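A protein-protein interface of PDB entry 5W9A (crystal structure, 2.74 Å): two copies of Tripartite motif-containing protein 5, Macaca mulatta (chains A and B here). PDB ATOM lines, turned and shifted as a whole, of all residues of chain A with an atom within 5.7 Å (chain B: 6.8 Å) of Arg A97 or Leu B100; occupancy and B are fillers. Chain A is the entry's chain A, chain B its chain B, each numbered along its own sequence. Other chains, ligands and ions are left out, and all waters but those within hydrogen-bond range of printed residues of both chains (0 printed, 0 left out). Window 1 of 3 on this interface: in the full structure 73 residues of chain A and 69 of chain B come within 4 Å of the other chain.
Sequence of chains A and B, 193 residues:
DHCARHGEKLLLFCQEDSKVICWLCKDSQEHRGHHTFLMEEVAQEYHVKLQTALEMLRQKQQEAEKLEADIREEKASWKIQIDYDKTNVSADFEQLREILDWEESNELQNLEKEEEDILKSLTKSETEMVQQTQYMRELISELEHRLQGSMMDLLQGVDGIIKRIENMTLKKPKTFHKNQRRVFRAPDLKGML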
ATOM      1  N   SER A  90      -0.202 -18.346 -18.712  1.00  0.00           N
ATOM      2  CA  SER A  90      -0.027 -19.267 -17.593  1.00  0.00           C
ATOM      3  C   SER A  90       0.863 -18.660 -16.513  1.00  0.00           C
ATOM      4  O   SER A  90       0.592 -18.811 -15.314  1.00  0.00           O
ATOM      5  CB  SER A  90       0.550 -20.593 -18.087  1.00  0.00           C
ATOM      6  OG  SER A  90       1.890 -20.437 -18.516  1.00  0.00           O
ATOM      7  N   ASP A  92       1.236 -15.437 -15.837  1.00  0.00           N
ATOM      8  CA  ASP A  92       0.479 -14.400 -15.136  1.00  0.00           C
ATOM      9  C   ASP A  92      -0.477 -15.011 -14.115  1.00  0.00           C
ATOM     10  O   ASP A  92      -0.599 -14.516 -12.983  1.00  0.00           O
ATOM     11  CB  ASP A  92      -0.284 -13.535 -16.138  1.00  0.00           C
ATOM     12  CG  ASP A  92       0.630 -12.626 -16.938  1.00  0.00           C
ATOM     13  OD1 ASP A  92       1.827 -12.532 -16.595  1.00  0.00           O
ATOM     14  OD2 ASP A  92       0.150 -12.004 -17.908  1.00  0.00           O
ATOM     15  N   PHE A  93      -1.165 -16.091 -14.496  1.00  0.00           N
ATOM     16  CA  PHE A  93      -2.062 -16.745 -13.547  1.00  0.00           C
ATOM     17  C   PHE A  93      -1.290 -17.329 -12.366  1.00  0.00           C
ATOM     18  O   PHE A  93      -1.770 -17.301 -11.225  1.00  0.00           O
ATOM     19  CB  PHE A  93      -2.886 -17.822 -14.253  1.00  0.00           C
ATOM     20  CG  PHE A  93      -4.172 -17.306 -14.836  1.00  0.00           C
ATOM     21  CD1 PHE A  93      -5.270 -17.076 -14.024  1.00  0.00           C
ATOM     22  CD2 PHE A  93      -4.277 -17.036 -16.190  1.00  0.00           C
ATOM     23  CE1 PHE A  93      -6.452 -16.595 -14.551  1.00  0.00           C
ATOM     24  CE2 PHE A  93      -5.459 -16.555 -16.723  1.00  0.00           C
ATOM     25  CZ  PHE A  93      -6.547 -16.333 -15.902  1.00  0.00           C
ATOM     26  N   GLU A  94      -0.081 -17.843 -12.615  1.00  0.00           N
ATOM     27  CA  GLU A  94       0.739 -18.344 -11.514  1.00  0.00           C
ATOM     28  C   GLU A  94       1.148 -17.219 -10.567  1.00  0.00           C
ATOM     29  O   GLU A  94       1.166 -17.403  -9.344  1.00  0.00           O
ATOM     30  CB  GLU A  94       1.973 -19.057 -12.064  1.00  0.00           C
ATOM     31  CG  GLU A  94       2.690 -19.927 -11.043  1.00  0.00           C
ATOM     32  CD  GLU A  94       1.833 -21.074 -10.546  1.00  0.00           C
ATOM     33  OE1 GLU A  94       1.014 -21.593 -11.334  1.00  0.00           O
ATOM     34  OE2 GLU A  94       1.977 -21.456  -9.366  1.00  0.00           O
ATOM     35  N   GLN A  95       1.486 -16.050 -11.117  1.00  0.00           N
ATOM     36  CA  GLN A  95       1.795 -14.892 -10.280  1.00  0.00           C
ATOM     37  C   GLN A  95       0.611 -14.525  -9.390  1.00  0.00           C
ATOM     38  O   GLN A  95       0.769 -14.269  -8.183  1.00  0.00           O
ATOM     39  CB  GLN A  95       2.192 -13.708 -11.163  1.00  0.00           C
ATOM     40  CG  GLN A  95       2.433 -12.414 -10.405  1.00  0.00           C
ATOM     41  CD  GLN A  95       3.773 -12.396  -9.702  1.00  0.00           C
ATOM     42  OE1 GLN A  95       4.825 -12.427 -10.344  1.00  0.00           O
ATOM     43  NE2 GLN A  95       3.747 -12.350  -8.375  1.00  0.00           N
ATOM     44  N   LEU A  96      -0.587 -14.474  -9.981  1.00  0.00           N
ATOM     45  CA  LEU A  96      -1.784 -14.179  -9.196  1.00  0.00           C
ATOM     46  C   LEU A  96      -1.985 -15.205  -8.085  1.00  0.00           C
ATOM     47  O   LEU A  96      -2.289 -14.843  -6.939  1.00  0.00           O
ATOM     48  CB  LEU A  96      -3.010 -14.128 -10.106  1.00  0.00           C
ATOM     49  CG  LEU A  96      -3.144 -12.876 -10.976  1.00  0.00           C
ATOM     50  CD1 LEU A  96      -4.290 -13.022 -11.968  1.00  0.00           C
ATOM     51  CD2 LEU A  96      -3.328 -11.640 -10.111  1.00  0.00           C
ATOM     52  N   ARG A  97      -1.804 -16.489  -8.402  1.00  0.00           N
ATOM     53  CA  ARG A  97      -1.980 -17.532  -7.395  1.00  0.00           C
ATOM     54  C   ARG A  97      -0.965 -17.386  -6.264  1.00  0.00           C
ATOM     55  O   ARG A  97      -1.288 -17.619  -5.091  1.00  0.00           O
ATOM     56  CB  ARG A  97      -1.873 -18.909  -8.052  1.00  0.00           C
ATOM     57  CG  ARG A  97      -2.598 -20.021  -7.310  1.00  0.00           C
ATOM     58  CD  ARG A  97      -2.820 -21.239  -8.201  1.00  0.00           C
ATOM     59  NE  ARG A  97      -3.762 -20.973  -9.287  1.00  0.00           N
ATOM     60  CZ  ARG A  97      -3.431 -20.928 -10.574  1.00  0.00           C
ATOM     61  NH1 ARG A  97      -2.175 -21.134 -10.945  1.00  0.00           N
ATOM     62  NH2 ARG A  97      -4.355 -20.678 -11.492  1.00  0.00           N
ATOM     63  N   GLU A  98       0.264 -16.982  -6.594  1.00  0.00           N
ATOM     64  CA  GLU A  98       1.290 -16.806  -5.569  1.00  0.00           C
ATOM     65  C   GLU A  98       0.940 -15.662  -4.622  1.00  0.00           C
ATOM     66  O   GLU A  98       1.046 -15.801  -3.393  1.00  0.00           O
ATOM     67  CB  GLU A  98       2.649 -16.565  -6.227  1.00  0.00           C
ATOM     68  CG  GLU A  98       3.311 -17.819  -6.772  1.00  0.00           C
ATOM     69  CD  GLU A  98       3.878 -18.700  -5.676  1.00  0.00           C
ATOM     70  OE1 GLU A  98       4.092 -18.190  -4.556  1.00  0.00           O
ATOM     71  OE2 GLU A  98       4.108 -19.901  -5.932  1.00  0.00           O
ATOM     72  N   ILE A  99       0.527 -14.518  -5.174  1.00  0.00           N
ATOM     73  CA  ILE A  99       0.177 -13.412  -4.282  1.00  0.00           C
ATOM     74  C   ILE A  99      -1.066 -13.757  -3.462  1.00  0.00           C
ATOM     75  O   ILE A  99      -1.204 -13.318  -2.308  1.00  0.00           O
ATOM     76  CB  ILE A  99       0.005 -12.093  -5.066  1.00  0.00           C
ATOM     77  CG1 ILE A  99      -1.342 -12.045  -5.790  1.00  0.00           C
ATOM     78  CG2 ILE A  99       1.162 -11.895  -6.039  1.00  0.00           C
ATOM     79  CD1 ILE A  99      -1.660 -10.690  -6.385  1.00  0.00           C
ATOM     80  N   LEU A 100      -1.965 -14.578  -4.014  1.00  0.00           N
ATOM     81  CA  LEU A 100      -3.113 -15.044  -3.242  1.00  0.00           C
ATOM     82  C   LEU A 100      -2.670 -15.904  -2.063  1.00  0.00           C
ATOM     83  O   LEU A 100      -3.188 -15.762  -0.947  1.00  0.00           O
ATOM     84  CB  LEU A 100      -4.065 -15.816  -4.155  1.00  0.00           C
ATOM     85  CG  LEU A 100      -5.483 -16.085  -3.657  1.00  0.00           C
ATOM     86  CD1 LEU A 100      -6.217 -14.776  -3.427  1.00  0.00           C
ATOM     87  CD2 LEU A 100      -6.233 -16.954  -4.653  1.00  0.00           C
ATOM     88  N   ASP A 101      -1.722 -16.816  -2.302  1.00  0.00           N
ATOM     89  CA  ASP A 101      -1.161 -17.618  -1.217  1.00  0.00           C
ATOM     90  C   ASP A 101      -0.576 -16.731  -0.124  1.00  0.00           C
ATOM     91  O   ASP A 101      -0.788 -16.975   1.074  1.00  0.00           O
ATOM     92  CB  ASP A 101      -0.086 -18.557  -1.764  1.00  0.00           C
ATOM     93  CG  ASP A 101      -0.661 -19.689  -2.592  1.00  0.00           C
ATOM     94  OD1 ASP A 101      -1.823 -20.077  -2.353  1.00  0.00           O
ATOM     95  OD2 ASP A 101       0.052 -20.189  -3.488  1.00  0.00           O
ATOM     96  N   TRP A 102       0.171 -15.697  -0.520  1.00  0.00           N
ATOM     97  CA  TRP A 102       0.784 -14.815   0.471  1.00  0.00           C
ATOM     98  C   TRP A 102      -0.273 -14.088   1.298  1.00  0.00           C
ATOM     99  O   TRP A 102      -0.138 -13.964   2.525  1.00  0.00           O
ATOM    100  CB  TRP A 102       1.719 -13.817  -0.211  1.00  0.00           C
ATOM    101  CG  TRP A 102       3.066 -14.387  -0.540  1.00  0.00           C
ATOM    102  CD1 TRP A 102       3.473 -14.895  -1.739  1.00  0.00           C
ATOM    103  CD2 TRP A 102       4.186 -14.509   0.347  1.00  0.00           C
ATOM    104  NE1 TRP A 102       4.777 -15.324  -1.654  1.00  0.00           N
ATOM    105  CE2 TRP A 102       5.235 -15.099  -0.383  1.00  0.00           C
ATOM    106  CE3 TRP A 102       4.401 -14.175   1.687  1.00  0.00           C
ATOM    107  CZ2 TRP A 102       6.483 -15.359   0.180  1.00  0.00           C
ATOM    108  CZ3 TRP A 102       5.641 -14.437   2.246  1.00  0.00           C
ATOM    109  CH2 TRP A 102       6.666 -15.022   1.492  1.00  0.00           C
ATOM    110  N   GLU B  94      -9.657 -20.791  -0.943  1.00  0.00           N
ATOM    111  CA  GLU B  94      -9.700 -21.930  -1.855  1.00  0.00           C
ATOM    112  C   GLU B  94     -10.746 -21.724  -2.948  1.00  0.00           C
ATOM    113  O   GLU B  94     -10.528 -22.100  -4.107  1.00  0.00           O
ATOM    114  CB  GLU B  94      -9.975 -23.216  -1.077  1.00  0.00           C
ATOM    115  CG  GLU B  94      -9.638 -24.478  -1.848  1.00  0.00           C
ATOM    116  CD  GLU B  94      -8.158 -24.583  -2.162  1.00  0.00           C
ATOM    117  OE1 GLU B  94      -7.340 -24.113  -1.341  1.00  0.00           O
ATOM    118  OE2 GLU B  94      -7.810 -25.128  -3.230  1.00  0.00           O
ATOM    119  N   GLN B  95     -11.894 -21.145  -2.590  1.00  0.00           N
ATOM    120  CA  GLN B  95     -12.903 -20.796  -3.588  1.00  0.00           C
ATOM    121  C   GLN B  95     -12.330 -19.845  -4.632  1.00  0.00           C
ATOM    122  O   GLN B  95     -12.539 -20.019  -5.845  1.00  0.00           O
ATOM    123  CB  GLN B  95     -14.116 -20.169  -2.898  1.00  0.00           C
ATOM    124  CG  GLN B  95     -15.182 -19.650  -3.847  1.00  0.00           C
ATOM    125  CD  GLN B  95     -16.032 -20.758  -4.428  1.00  0.00           C
ATOM    126  OE1 GLN B  95     -16.756 -21.443  -3.707  1.00  0.00           O
ATOM    127  NE2 GLN B  95     -15.952 -20.939  -5.741  1.00  0.00           N
ATOM    128  N   LEU B  96     -11.620 -18.812  -4.170  1.00  0.00           N
ATOM    129  CA  LEU B  96     -10.978 -17.884  -5.099  1.00  0.00           C
ATOM    130  C   LEU B  96     -10.004 -18.612  -6.020  1.00  0.00           C
ATOM    131  O   LEU B  96      -9.970 -18.356  -7.231  1.00  0.00           O
ATOM    132  CB  LEU B  96     -10.263 -16.775  -4.329  1.00  0.00           C
ATOM    133  CG  LEU B  96     -11.150 -15.689  -3.720  1.00  0.00           C
ATOM    134  CD1 LEU B  96     -10.336 -14.764  -2.826  1.00  0.00           C
ATOM    135  CD2 LEU B  96     -11.855 -14.901  -4.816  1.00  0.00           C
ATOM    136  N   ARG B  97      -9.209 -19.528  -5.464  1.00  0.00           N
ATOM    137  CA  ARG B  97      -8.247 -20.270  -6.276  1.00  0.00           C
ATOM    138  C   ARG B  97      -8.951 -21.128  -7.327  1.00  0.00           C
ATOM    139  O   ARG B  97      -8.476 -21.253  -8.466  1.00  0.00           O
ATOM    140  CB  ARG B  97      -7.369 -21.132  -5.368  1.00  0.00           C
ATOM    141  CG  ARG B  97      -6.004 -21.474  -5.937  1.00  0.00           C
ATOM    142  CD  ARG B  97      -5.059 -21.939  -4.836  1.00  0.00           C
ATOM    143  NE  ARG B  97      -4.724 -20.861  -3.909  1.00  0.00           N
ATOM    144  CZ  ARG B  97      -5.118 -20.812  -2.641  1.00  0.00           C
ATOM    145  NH1 ARG B  97      -5.865 -21.785  -2.137  1.00  0.00           N
ATOM    146  NH2 ARG B  97      -4.766 -19.789  -1.872  1.00  0.00           N
ATOM    147  N   GLU B  98     -10.097 -21.710  -6.969  1.00  0.00           N
ATOM    148  CA  GLU B  98     -10.841 -22.539  -7.915  1.00  0.00           C
ATOM    149  C   GLU B  98     -11.376 -21.704  -9.073  1.00  0.00           C
ATOM    150  O   GLU B  98     -11.256 -22.091 -10.247  1.00  0.00           O
ATOM    151  CB  GLU B  98     -11.984 -23.254  -7.191  1.00  0.00           C
ATOM    152  CG  GLU B  98     -12.281 -24.656  -7.703  1.00  0.00           C
ATOM    153  CD  GLU B  98     -11.229 -25.666  -7.283  1.00  0.00           C
ATOM    154  OE1 GLU B  98     -10.395 -26.051  -8.129  1.00  0.00           O
ATOM    155  OE2 GLU B  98     -11.230 -26.069  -6.100  1.00  0.00           O
ATOM    156  N   ILE B  99     -11.977 -20.550  -8.766  1.00  0.00           N
ATOM    157  CA  ILE B  99     -12.482 -19.716  -9.856  1.00  0.00           C
ATOM    158  C   ILE B  99     -11.325 -19.176 -10.695  1.00  0.00           C
ATOM    159  O   ILE B  99     -11.475 -18.953 -11.906  1.00  0.00           O
ATOM    160  CB  ILE B  99     -13.388 -18.586  -9.326  1.00  0.00           C
ATOM    161  CG1 ILE B  99     -12.565 -17.444  -8.726  1.00  0.00           C
ATOM    162  CG2 ILE B  99     -14.389 -19.131  -8.317  1.00  0.00           C
ATOM    163  CD1 ILE B  99     -13.383 -16.214  -8.400  1.00  0.00           C
ATOM    164  N   LEU B 100     -10.152 -18.989 -10.084  1.00  0.00           N
ATOM    165  CA  LEU B 100      -8.971 -18.593 -10.847  1.00  0.00           C
ATOM    166  C   LEU B 100      -8.582 -19.675 -11.848  1.00  0.00           C
ATOM    167  O   LEU B 100      -8.275 -19.383 -13.012  1.00  0.00           O
ATOM    168  CB  LEU B 100      -7.815 -18.301  -9.890  1.00  0.00           C
ATOM    169  CG  LEU B 100      -6.599 -17.553 -10.436  1.00  0.00           C
ATOM    170  CD1 LEU B 100      -6.994 -16.167 -10.917  1.00  0.00           C
ATOM    171  CD2 LEU B 100      -5.508 -17.468  -9.378  1.00  0.00           C
ATOM    172  N   ASP B 101      -8.581 -20.935 -11.404  1.00  0.00           N
ATOM    173  CA  ASP B 101      -8.328 -22.047 -12.321  1.00  0.00           C
ATOM    174  C   ASP B 101      -9.324 -22.051 -13.474  1.00  0.00           C
ATOM    175  O   ASP B 101      -8.944 -22.259 -14.636  1.00  0.00           O
ATOM    176  CB  ASP B 101      -8.378 -23.379 -11.572  1.00  0.00           C
ATOM    177  CG  ASP B 101      -7.169 -23.598 -10.688  1.00  0.00           C
ATOM    178  OD1 ASP B 101      -6.094 -23.044 -11.000  1.00  0.00           O
ATOM    179  OD2 ASP B 101      -7.290 -24.332  -9.684  1.00  0.00           O
ATOM    180  N   TRP B 102     -10.608 -21.839 -13.171  1.00  0.00           N
ATOM    181  CA  TRP B 102     -11.618 -21.859 -14.230  1.00  0.00           C
ATOM    182  C   TRP B 102     -11.386 -20.745 -15.249  1.00  0.00           C
ATOM    183  O   TRP B 102     -11.480 -20.972 -16.464  1.00  0.00           O
ATOM    184  CB  TRP B 102     -13.021 -21.756 -13.631  1.00  0.00           C
ATOM    185  CG  TRP B 102     -13.547 -23.059 -13.107  1.00  0.00           C
ATOM    186  CD1 TRP B 102     -13.522 -23.495 -11.814  1.00  0.00           C
ATOM    187  CD2 TRP B 102     -14.173 -24.099 -13.869  1.00  0.00           C
ATOM    188  NE1 TRP B 102     -14.096 -24.740 -11.723  1.00  0.00           N
ATOM    189  CE2 TRP B 102     -14.504 -25.133 -12.971  1.00  0.00           C
ATOM    190  CE3 TRP B 102     -14.489 -24.254 -15.221  1.00  0.00           C
ATOM    191  CZ2 TRP B 102     -15.134 -26.305 -13.382  1.00  0.00           C
ATOM    192  CZ3 TRP B 102     -15.114 -25.420 -15.628  1.00  0.00           C
ATOM    193  CH2 TRP B 102     -15.430 -26.430 -14.711  1.00  0.00           C
ATOM    194  N   GLU B 103     -11.078 -19.535 -14.774  1.00  0.00           N
ATOM    195  CA  GLU B 103     -10.816 -18.432 -15.698  1.00  0.00           C
ATOM    196  C   GLU B 103      -9.580 -18.704 -16.550  1.00  0.00           C
ATOM    197  O   GLU B 103      -9.557 -18.388 -17.750  1.00  0.00           O
ATOM    198  CB  GLU B 103     -10.663 -17.123 -14.923  1.00  0.00           C
ATOM    199  CG  GLU B 103     -11.968 -16.583 -14.358  1.00  0.00           C
ATOM    200  CD  GLU B 103     -12.889 -16.026 -15.431  1.00  0.00           C
ATOM    201  OE1 GLU B 103     -12.408 -15.757 -16.553  1.00  0.00           O
ATOM    202  OE2 GLU B 103     -14.094 -15.857 -15.151  1.00  0.00           O
ATOM    203  N   GLU B 104      -8.536 -19.279 -15.945  1.00  0.00           N
ATOM    204  CA  GLU B 104      -7.345 -19.636 -16.709  1.00  0.00           C
ATOM    205  C   GLU B 104      -7.679 -20.629 -17.815  1.00  0.00           C
ATOM    206  O   GLU B 104      -7.218 -20.483 -18.955  1.00  0.00           O
ATOM    207  CB  GLU B 104      -6.276 -20.204 -15.774  1.00  0.00           C
ATOM    208  CG  GLU B 104      -5.053 -20.757 -16.485  1.00  0.00           C
ATOM    209  CD  GLU B 104      -4.096 -21.454 -15.537  1.00  0.00           C
ATOM    210  OE1 GLU B 104      -4.349 -21.433 -14.313  1.00  0.00           O
ATOM    211  OE2 GLU B 104      -3.091 -22.021 -16.014  1.00  0.00           O
ATOM    212  N   SER B 105      -8.476 -21.652 -17.493  1.00  0.00           N
ATOM    213  CA  SER B 105      -8.872 -22.627 -18.506  1.00  0.00           C
ATOM    214  C   SER B 105      -9.662 -21.966 -19.630  1.00  0.00           C
ATOM    215  O   SER B 105      -9.465 -22.286 -20.811  1.00  0.00           O
ATOM    216  CB  SER B 105      -9.688 -23.748 -17.863  1.00  0.00           C
ATOM    217  OG  SER B 105      -9.954 -24.782 -18.794  1.00  0.00           O
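NH2 of Arg A97 lies within salt-bridge range of OE1 of Glu B104. The side-chain carboxylate of Asp A101 is in salt-bridge range of the guanidinium group of Arg B97 (3.0 Å). NH2 of Arg A97 lies within salt-bridge range of OD1 of Asp B101, 3.0 Å away.
The side-chain carboxylate (OE1) of Glu B94 lies within salt-bridge range of the guanidinium group (NH1) of Arg B97 (2.9 Å). NH1 of Arg A97 lies within salt-bridge range of OE1 of Glu A94 (3.2 Å).
Among the printed residues, pairs that only touch across the chains: Phe A93 with Leu B100, Phe A93 with Glu B103, Phe A93 with Glu B104, Arg A97 with Arg B97 and Arg A97 with Leu B100.
Printed residues of chain B within 4 Å of Phe A93: Leu B100 (3.7 Å), Glu B103 (3.9 Å) and Glu B104 (3.5 Å). Arg A97 touches four residues of chain B. Glu B98 touches none of the printed residues of chain A. Leu B100 touches two residues of chain A. Of the printed residues of chain A, Asp B101 touches Arg A97. Of the printed residues of chain A, Glu B103 touches Phe A93. The nearest printed residue of chain A that does not touch Glu B104 is Ser A90 (4.4 Å).
Printed residues of chain A that touch a printed residue of chain B: Phe A93, Arg A97 and Asp A101. Hydrophobic or aromatic side chains of chain A that line the printed part of chain B: Phe A93. Of the 12 printed residues of chain B, 5 touch a printed residue of chain A. Hydrophobic or aromatic side chains of chain B that line the printed part of chain A: Leu B100. Among the printed residues, Asp or Glu carboxylates within 4 Å of a Lys or Arg side-chain nitrogen of the other chain: Arg A97 with Asp B101, Arg A97 with Glu B104 and Asp A101 with Arg B97.
Arg B97 touches its own counterpart, Arg A97. Arg A97 touches Leu B100, but with the chains exchanged Leu A100 does not touch Arg B97 (4.02 Å). Arg A97 touches Asp B101, and with the chains exchanged Asp A101 touches Arg B97. Positions printed for both chains: 94, 95, 96, 97, 98, 99, 100, 101 and 102. Of the 8 pairs that touch across the chains among the printed residues, 3 have their exchanged pair printed and touching as well.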
